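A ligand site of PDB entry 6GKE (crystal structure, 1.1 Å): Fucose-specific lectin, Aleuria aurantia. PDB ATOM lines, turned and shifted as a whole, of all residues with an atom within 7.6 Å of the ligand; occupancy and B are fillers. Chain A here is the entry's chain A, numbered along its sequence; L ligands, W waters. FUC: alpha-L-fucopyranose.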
ATOM      1  N   ILE A  13      12.862  16.885  -8.444  1.00  0.00           N
ATOM      2  CA  ILE A  13      12.917  15.443  -8.216  1.00  0.00           C
ATOM      3  C   ILE A  13      14.290  15.090  -7.621  1.00  0.00           C
ATOM      4  O   ILE A  13      15.254  15.837  -7.750  1.00  0.00           O
ATOM      5  CB  ILE A  13      12.652  14.652  -9.514  1.00  0.00           C
ATOM      6  CG1 ILE A  13      13.657  15.032 -10.611  1.00  0.00           C
ATOM      7  CG2 ILE A  13      11.202  14.803  -9.955  1.00  0.00           C
ATOM      8  CD1 ILE A  13      13.583  14.195 -11.865  1.00  0.00           C
ATOM      9  N   TRP A  15      16.678  11.243  -6.519  1.00  0.00           N
ATOM     10  CA  TRP A  15      16.759   9.807  -6.352  1.00  0.00           C
ATOM     11  C   TRP A  15      18.115   9.424  -5.782  1.00  0.00           C
ATOM     12  O   TRP A  15      19.121  10.088  -5.998  1.00  0.00           O
ATOM     13  CB  TRP A  15      16.443   9.048  -7.655  1.00  0.00           C
ATOM     14  CG  TRP A  15      17.398   9.260  -8.793  1.00  0.00           C
ATOM     15  CD1 TRP A  15      18.444   8.470  -9.155  1.00  0.00           C
ATOM     16  CD2 TRP A  15      17.336  10.309  -9.767  1.00  0.00           C
ATOM     17  NE1 TRP A  15      19.045   8.959 -10.274  1.00  0.00           N
ATOM     18  CE2 TRP A  15      18.400  10.090 -10.677  1.00  0.00           C
ATOM     19  CE3 TRP A  15      16.517  11.433  -9.967  1.00  0.00           C
ATOM     20  CZ2 TRP A  15      18.651  10.940 -11.749  1.00  0.00           C
ATOM     21  CZ3 TRP A  15      16.768  12.272 -11.025  1.00  0.00           C
ATOM     22  CH2 TRP A  15      17.817  12.031 -11.909  1.00  0.00           C
ATOM     23  N   GLN A  22      21.045  12.077  -6.732  1.00  0.00           N
ATOM     24  CA  GLN A  22      20.863  12.880  -7.932  1.00  0.00           C
ATOM     25  C   GLN A  22      19.609  13.733  -7.756  1.00  0.00           C
ATOM     26  O   GLN A  22      18.574  13.229  -7.338  1.00  0.00           O
ATOM     27  CB  GLN A  22      20.726  11.983  -9.155  1.00  0.00           C
ATOM     28  CG  GLN A  22      22.025  11.307  -9.564  1.00  0.00           C
ATOM     29  CD  GLN A  22      23.059  12.252 -10.139  1.00  0.00           C
ATOM     30  OE1 GLN A  22      22.726  13.223 -10.807  1.00  0.00           O
ATOM     31  NE2 GLN A  22      24.322  11.978  -9.893  1.00  0.00           N
ATOM     32  N   GLN A  23      19.715  15.018  -8.090  1.00  0.00           N
ATOM     33  CA  GLN A  23      18.587  15.917  -8.081  1.00  0.00           C
ATOM     34  C   GLN A  23      18.446  16.565  -9.462  1.00  0.00           C
ATOM     35  O   GLN A  23      19.442  16.837 -10.142  1.00  0.00           O
ATOM     36  CB  GLN A  23      18.762  17.043  -7.065  1.00  0.00           C
ATOM     37  CG  GLN A  23      18.836  16.577  -5.629  1.00  0.00           C
ATOM     38  CD  GLN A  23      18.967  17.766  -4.719  1.00  0.00           C
ATOM     39  OE1 GLN A  23      17.993  18.482  -4.474  1.00  0.00           O
ATOM     40  NE2 GLN A  23      20.166  17.985  -4.212  1.00  0.00           N
ATOM     41  N   ARG A  24      17.203  16.836  -9.851  1.00  0.00           N
ATOM     42  CA  ARG A  24      16.928  17.678 -10.999  1.00  0.00           C
ATOM     43  C   ARG A  24      15.890  18.707 -10.578  1.00  0.00           C
ATOM     44  O   ARG A  24      14.956  18.400  -9.850  1.00  0.00           O
ATOM     45  CB  ARG A  24      16.399  16.889 -12.201  1.00  0.00           C
ATOM     46  CG  ARG A  24      17.271  15.709 -12.638  1.00  0.00           C
ATOM     47  CD  ARG A  24      18.573  16.144 -13.280  1.00  0.00           C
ATOM     48  NE  ARG A  24      19.387  15.015 -13.738  1.00  0.00           N
ATOM     49  CZ  ARG A  24      20.284  14.358 -13.004  1.00  0.00           C
ATOM     50  NH1 ARG A  24      20.545  14.744 -11.758  1.00  0.00           N
ATOM     51  NH2 ARG A  24      20.919  13.315 -13.517  1.00  0.00           N
ATOM     52  N   TYR A  26      13.468  21.938 -12.356  1.00  0.00           N
ATOM     53  CA  TYR A  26      12.881  22.465 -13.584  1.00  0.00           C
ATOM     54  C   TYR A  26      12.299  23.845 -13.287  1.00  0.00           C
ATOM     55  O   TYR A  26      11.639  24.053 -12.268  1.00  0.00           O
ATOM     56  CB  TYR A  26      11.806  21.515 -14.141  1.00  0.00           C
ATOM     57  CG  TYR A  26      12.390  20.156 -14.391  1.00  0.00           C
ATOM     58  CD1 TYR A  26      13.134  19.903 -15.524  1.00  0.00           C
ATOM     59  CD2 TYR A  26      12.314  19.164 -13.427  1.00  0.00           C
ATOM     60  CE1 TYR A  26      13.773  18.695 -15.718  1.00  0.00           C
ATOM     61  CE2 TYR A  26      12.945  17.941 -13.596  1.00  0.00           C
ATOM     62  CZ  TYR A  26      13.688  17.715 -14.737  1.00  0.00           C
ATOM     63  OH  TYR A  26      14.362  16.540 -14.873  1.00  0.00           O
ATOM     64  N   GLU A  36      16.450  22.594 -17.164  1.00  0.00           N
ATOM     65  CA  GLU A  36      16.832  21.675 -16.119  1.00  0.00           C
ATOM     66  C   GLU A  36      18.190  22.075 -15.542  1.00  0.00           C
ATOM     67  O   GLU A  36      19.111  22.403 -16.299  1.00  0.00           O
ATOM     68  CB  GLU A  36      16.942  20.256 -16.686  1.00  0.00           C
ATOM     69  CG  GLU A  36      17.180  19.163 -15.659  1.00  0.00           C
ATOM     70  CD  GLU A  36      17.491  17.833 -16.303  1.00  0.00           C
ATOM     71  OE1 GLU A  36      18.558  17.754 -16.959  1.00  0.00           O
ATOM     72  OE2 GLU A  36      16.683  16.884 -16.183  1.00  0.00           O
ATOM     73  N   ALA A  37      18.297  22.000 -14.213  1.00  0.00           N
ATOM     74  CA  ALA A  37      19.592  22.016 -13.502  1.00  0.00           C
ATOM     75  C   ALA A  37      19.740  20.673 -12.791  1.00  0.00           C
ATOM     76  O   ALA A  37      18.734  20.034 -12.436  1.00  0.00           O
ATOM     77  CB  ALA A  37      19.691  23.187 -12.549  1.00  0.00           C
ATOM     78  N   GLN A  38      20.995  20.247 -12.585  1.00  0.00           N
ATOM     79  CA  GLN A  38      21.300  18.919 -12.049  1.00  0.00           C
ATOM     80  C   GLN A  38      22.277  19.037 -10.890  1.00  0.00           C
ATOM     81  O   GLN A  38      23.166  19.892 -10.890  1.00  0.00           O
ATOM     82  CB  GLN A  38      21.946  18.026 -13.115  1.00  0.00           C
ATOM     83  CG  GLN A  38      21.255  18.048 -14.472  1.00  0.00           C
ATOM     84  CD  GLN A  38      21.666  19.178 -15.386  1.00  0.00           C
ATOM     85  OE1 GLN A  38      22.721  19.795 -15.239  1.00  0.00           O
ATOM     86  NE2 GLN A  38      20.816  19.457 -16.363  1.00  0.00           N
ATOM     87  N   THR A  46      24.958  21.885 -11.744  1.00  0.00           N
ATOM     88  CA  THR A  46      25.225  22.109 -13.148  1.00  0.00           C
ATOM     89  C   THR A  46      23.926  22.495 -13.869  1.00  0.00           C
ATOM     90  O   THR A  46      22.828  22.406 -13.305  1.00  0.00           O
ATOM     91  CB  THR A  46      25.856  20.869 -13.783  1.00  0.00           C
ATOM     92  OG1 THR A  46      24.973  19.746 -13.643  1.00  0.00           O
ATOM     93  CG2 THR A  46      27.198  20.519 -13.172  1.00  0.00           C
ATOM     94  N   ASN A  52      20.234  23.597 -21.733  1.00  0.00           N
ATOM     95  CA  ASN A  52      19.583  22.647 -20.822  1.00  0.00           C
ATOM     96  C   ASN A  52      18.068  22.722 -20.956  1.00  0.00           C
ATOM     97  O   ASN A  52      17.348  22.496 -19.977  1.00  0.00           O
ATOM     98  CB  ASN A  52      20.006  22.906 -19.376  1.00  0.00           C
ATOM     99  CG  ASN A  52      21.486  22.740 -19.169  1.00  0.00           C
ATOM    100  OD1 ASN A  52      22.210  23.721 -19.014  1.00  0.00           O
ATOM    101  ND2 ASN A  52      21.950  21.503 -19.206  1.00  0.00           N
ATOM    102  N   VAL A  53      17.572  23.003 -22.156  1.00  0.00           N
ATOM    103  CA  VAL A  53      16.140  23.061 -22.411  1.00  0.00           C
ATOM    104  C   VAL A  53      15.612  21.631 -22.594  1.00  0.00           C
ATOM    105  O   VAL A  53      16.167  20.851 -23.358  1.00  0.00           O
ATOM    106  CB  VAL A  53      15.841  23.940 -23.634  1.00  0.00           C
ATOM    107  CG1 VAL A  53      14.404  23.799 -24.095  1.00  0.00           C
ATOM    108  CG2 VAL A  53      16.188  25.392 -23.351  1.00  0.00           C
ATOM    109  N   ILE A  54      14.517  21.317 -21.892  1.00  0.00           N
ATOM    110  CA  ILE A  54      13.886  19.992 -21.949  1.00  0.00           C
ATOM    111  C   ILE A  54      12.494  20.052 -22.587  1.00  0.00           C
ATOM    112  O   ILE A  54      11.931  19.015 -22.907  1.00  0.00           O
ATOM    113  CB  ILE A  54      13.864  19.318 -20.558  1.00  0.00           C
ATOM    114  CG1 ILE A  54      12.932  19.986 -19.542  1.00  0.00           C
ATOM    115  CG2 ILE A  54      15.277  19.190 -20.033  1.00  0.00           C
ATOM    116  CD1 ILE A  54      11.486  19.591 -19.628  1.00  0.00           C
ATOM    117  N   THR A  67       9.715  10.981 -11.139  1.00  0.00           N
ATOM    118  CA  THR A  67      10.793  10.145 -11.663  1.00  0.00           C
ATOM    119  C   THR A  67      10.697   8.747 -11.056  1.00  0.00           C
ATOM    120  O   THR A  67      10.193   8.551  -9.957  1.00  0.00           O
ATOM    121  CB  THR A  67      12.153  10.793 -11.376  1.00  0.00           C
ATOM    122  OG1 THR A  67      13.206  10.080 -12.031  1.00  0.00           O
ATOM    123  CG2 THR A  67      12.488  10.849  -9.903  1.00  0.00           C
ATOM    124  N   GLY A  73      16.474   3.053 -18.155  1.00  0.00           N
ATOM    125  CA  GLY A  73      17.216   4.091 -17.450  1.00  0.00           C
ATOM    126  C   GLY A  73      16.300   4.935 -16.587  1.00  0.00           C
ATOM    127  O   GLY A  73      15.174   4.527 -16.259  1.00  0.00           O
ATOM    128  N   ILE A  74      16.784   6.113 -16.201  1.00  0.00           N
ATOM    129  CA  ILE A  74      16.003   7.028 -15.396  1.00  0.00           C
ATOM    130  C   ILE A  74      14.875   7.588 -16.253  1.00  0.00           C
ATOM    131  O   ILE A  74      15.117   8.145 -17.315  1.00  0.00           O
ATOM    132  CB  ILE A  74      16.886   8.157 -14.827  1.00  0.00           C
ATOM    133  CG1 ILE A  74      18.042   7.613 -13.972  1.00  0.00           C
ATOM    134  CG2 ILE A  74      16.045   9.153 -14.041  1.00  0.00           C
ATOM    135  CD1 ILE A  74      17.616   6.781 -12.789  1.00  0.00           C
ATOM    136  N   GLN A  75      13.645   7.444 -15.760  1.00  0.00           N
ATOM    137  CA  GLN A  75      12.472   8.034 -16.379  1.00  0.00           C
ATOM    138  C   GLN A  75      12.106   9.324 -15.635  1.00  0.00           C
ATOM    139  O   GLN A  75      12.059   9.344 -14.413  1.00  0.00           O
ATOM    140  CB  GLN A  75      11.291   7.067 -16.367  1.00  0.00           C
ATOM    141  CG  GLN A  75      11.553   5.764 -17.118  1.00  0.00           C
ATOM    142  CD  GLN A  75      11.366   5.869 -18.611  1.00  0.00           C
ATOM    143  OE1 GLN A  75      10.709   6.785 -19.120  1.00  0.00           O
ATOM    144  NE2 GLN A  75      11.948   4.921 -19.323  1.00  0.00           N
ATOM    145  N   ILE A  76      11.860  10.391 -16.394  1.00  0.00           N
ATOM    146  CA  ILE A  76      11.370  11.638 -15.830  1.00  0.00           C
ATOM    147  C   ILE A  76      10.141  12.051 -16.646  1.00  0.00           C
ATOM    148  O   ILE A  76      10.105  11.874 -17.864  1.00  0.00           O
ATOM    149  CB  ILE A  76      12.432  12.759 -15.825  1.00  0.00           C
ATOM    150  CG1 ILE A  76      13.720  12.292 -15.155  1.00  0.00           C
ATOM    151  CG2 ILE A  76      11.870  14.020 -15.179  1.00  0.00           C
ATOM    152  CD1 ILE A  76      14.912  13.192 -15.397  1.00  0.00           C
ATOM    153  N   TYR A  92      11.619  12.254 -20.285  1.00  0.00           N
ATOM    154  CA  TYR A  92      12.967  11.736 -20.410  1.00  0.00           C
ATOM    155  C   TYR A  92      12.835  10.219 -20.338  1.00  0.00           C
ATOM    156  O   TYR A  92      12.375   9.689 -19.327  1.00  0.00           O
ATOM    157  CB  TYR A  92      13.917  12.251 -19.325  1.00  0.00           C
ATOM    158  CG  TYR A  92      15.346  11.843 -19.566  1.00  0.00           C
ATOM    159  CD1 TYR A  92      16.115  12.480 -20.532  1.00  0.00           C
ATOM    160  CD2 TYR A  92      15.923  10.803 -18.863  1.00  0.00           C
ATOM    161  CE1 TYR A  92      17.428  12.111 -20.775  1.00  0.00           C
ATOM    162  CE2 TYR A  92      17.236  10.420 -19.103  1.00  0.00           C
ATOM    163  CZ  TYR A  92      17.989  11.075 -20.054  1.00  0.00           C
ATOM    164  OH  TYR A  92      19.279  10.703 -20.279  1.00  0.00           O
ATOM    165  N   GLY A  94      15.037   7.781 -20.450  1.00  0.00           N
ATOM    166  CA  GLY A  94      16.252   7.080 -20.067  1.00  0.00           C
ATOM    167  C   GLY A  94      17.455   7.522 -20.878  1.00  0.00           C
ATOM    168  O   GLY A  94      18.589   7.321 -20.437  1.00  0.00           O
ATOM    169  N   SER A  95      17.228   8.122 -22.056  1.00  0.00           N
ATOM    170  CA  SER A  95      18.340   8.559 -22.896  1.00  0.00           C
ATOM    171  C   SER A  95      18.089   9.909 -23.569  1.00  0.00           C
ATOM    172  O   SER A  95      19.060  10.589 -23.877  1.00  0.00           O
ATOM    173  CB  SER A  95      18.687   7.512 -23.919  1.00  0.00           C
ATOM    174  OG  SER A  95      17.607   7.291 -24.810  1.00  0.00           O
ATOM    175  N   LYS A  96      16.827  10.314 -23.768  1.00  0.00           N
ATOM    176  CA  LYS A  96      16.542  11.566 -24.469  1.00  0.00           C
ATOM    177  C   LYS A  96      15.221  12.165 -23.988  1.00  0.00           C
ATOM    178  O   LYS A  96      14.372  11.470 -23.443  1.00  0.00           O
ATOM    179  CB  LYS A  96      16.474  11.310 -25.982  1.00  0.00           C
ATOM    180  CG  LYS A  96      15.382  10.331 -26.407  1.00  0.00           C
ATOM    181  CD  LYS A  96      15.349  10.035 -27.884  1.00  0.00           C
ATOM    182  CE  LYS A  96      14.388   8.921 -28.236  1.00  0.00           C
ATOM    183  NZ  LYS A  96      14.757   7.638 -27.580  1.00  0.00           N
ATOM    184  N   TRP A  97      15.078  13.462 -24.248  1.00  0.00           N
ATOM    185  CA  TRP A  97      13.860  14.213 -23.997  1.00  0.00           C
ATOM    186  C   TRP A  97      13.003  14.240 -25.258  1.00  0.00           C
ATOM    187  O   TRP A  97      13.472  14.614 -26.328  1.00  0.00           O
ATOM    188  CB  TRP A  97      14.188  15.628 -23.560  1.00  0.00           C
ATOM    189  CG  TRP A  97      14.726  15.727 -22.171  1.00  0.00           C
ATOM    190  CD1 TRP A  97      16.031  15.799 -21.778  1.00  0.00           C
ATOM    191  CD2 TRP A  97      13.943  15.715 -20.956  1.00  0.00           C
ATOM    192  NE1 TRP A  97      16.119  15.858 -20.416  1.00  0.00           N
ATOM    193  CE2 TRP A  97      14.858  15.806 -19.879  1.00  0.00           C
ATOM    194  CE3 TRP A  97      12.578  15.657 -20.679  1.00  0.00           C
ATOM    195  CZ2 TRP A  97      14.438  15.861 -18.560  1.00  0.00           C
ATOM    196  CZ3 TRP A  97      12.166  15.702 -19.368  1.00  0.00           C
ATOM    197  CH2 TRP A  97      13.076  15.805 -18.326  1.00  0.00           C
HETATM  198  C1  FUC L   1      21.249  13.636 -17.220  1.00  0.00           C
HETATM  199  C2  FUC L   1      20.584  14.903 -17.737  1.00  0.00           C
HETATM  200  C3  FUC L   1      19.223  14.581 -18.347  1.00  0.00           C
HETATM  201  C4  FUC L   1      18.376  13.787 -17.355  1.00  0.00           C
HETATM  202  C5  FUC L   1      19.134  12.542 -16.929  1.00  0.00           C
HETATM  203  C6  FUC L   1      18.396  11.693 -15.911  1.00  0.00           C
HETATM  204  O1  FUC L   1      21.602  12.853 -18.350  1.00  0.00           O
HETATM  205  O2  FUC L   1      21.417  15.486 -18.743  1.00  0.00           O
HETATM  206  O3  FUC L   1      18.574  15.783 -18.759  1.00  0.00           O
HETATM  207  O4  FUC L   1      18.078  14.555 -16.184  1.00  0.00           O
HETATM  208  O5  FUC L   1      20.378  12.940 -16.343  1.00  0.00           O
HETATM  209  O   HOH W   1      22.355  17.893 -19.190  1.00  0.00           O
HETATM  210  O   HOH W   2      22.560  14.202 -20.700  1.00  0.00           O
HETATM  211  O   HOH W   3      20.773  12.494 -21.714  1.00  0.00           O
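The indole nitrogen (NE1) of Trp 97 is in hydrogen-bond range of an oxygen (O3) of the ligand.
The guanidinium group of Arg 24 is in hydrogen-bond range of an oxygen (O4) of the ligand, 2.8 Å away.
OE1 of Glu 36 is in hydrogen-bond range of O3 of the ligand (2.7 Å).
The backbone carbonyl oxygen (O) of Tyr 92 sits close to the side-chain amide oxygen (OE1) of Gln 75, at 3.4 Å.
The side-chain carboxylate (OE1) of Glu 36 sits at hydrogen-bond distance from the side-chain amide nitrogen (NE2) of Gln 38 (2.9 Å).
The backbone carbonyl oxygen (O) of Asn 52 lies within hydrogen-bond range of the backbone NH (N) of Glu 36 (3.0 Å).
The side-chain carboxylate (OE2) of Glu 36 sits at hydrogen-bond distance from the side-chain hydroxyl (OH) of Tyr 26 (2.7 Å).
The backbone NH of Ile 13 sits at hydrogen-bond distance from the backbone carbonyl oxygen of Arg 24, 2.9 Å away.
OH of Tyr 92 sits at hydrogen-bond distance from O of Gly 94.
The backbone NH (N) of Tyr 92 sits at hydrogen-bond distance from the backbone carbonyl oxygen (O) of Ile 76.
NH1 of Arg 24 sits at hydrogen-bond distance from OE1 of Gln 22 (2.8 Å).
Ile 74 touches the ligand.
Ile 76 touches the ligand.
Tyr 92 touches the ligand (CE2 to C5, 3.6 Å).
Hydrophobic or aromatic side chains that line the ligand: Ile 74, Ile 76, Tyr 92 and Trp 97.
Within 4 Å of the ligand: Arg 24, Glu 36, Ile 74, Ile 76, Tyr 92 and Trp 97.
The nearest printed residue that does not touch the ligand is Trp 15 (4.1 Å).
Water W3 lies within hydrogen-bond range of OH of Tyr 92 (2.7 Å), O of Ser 95 (3.4 Å) and O1 of the ligand (3.5 Å).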
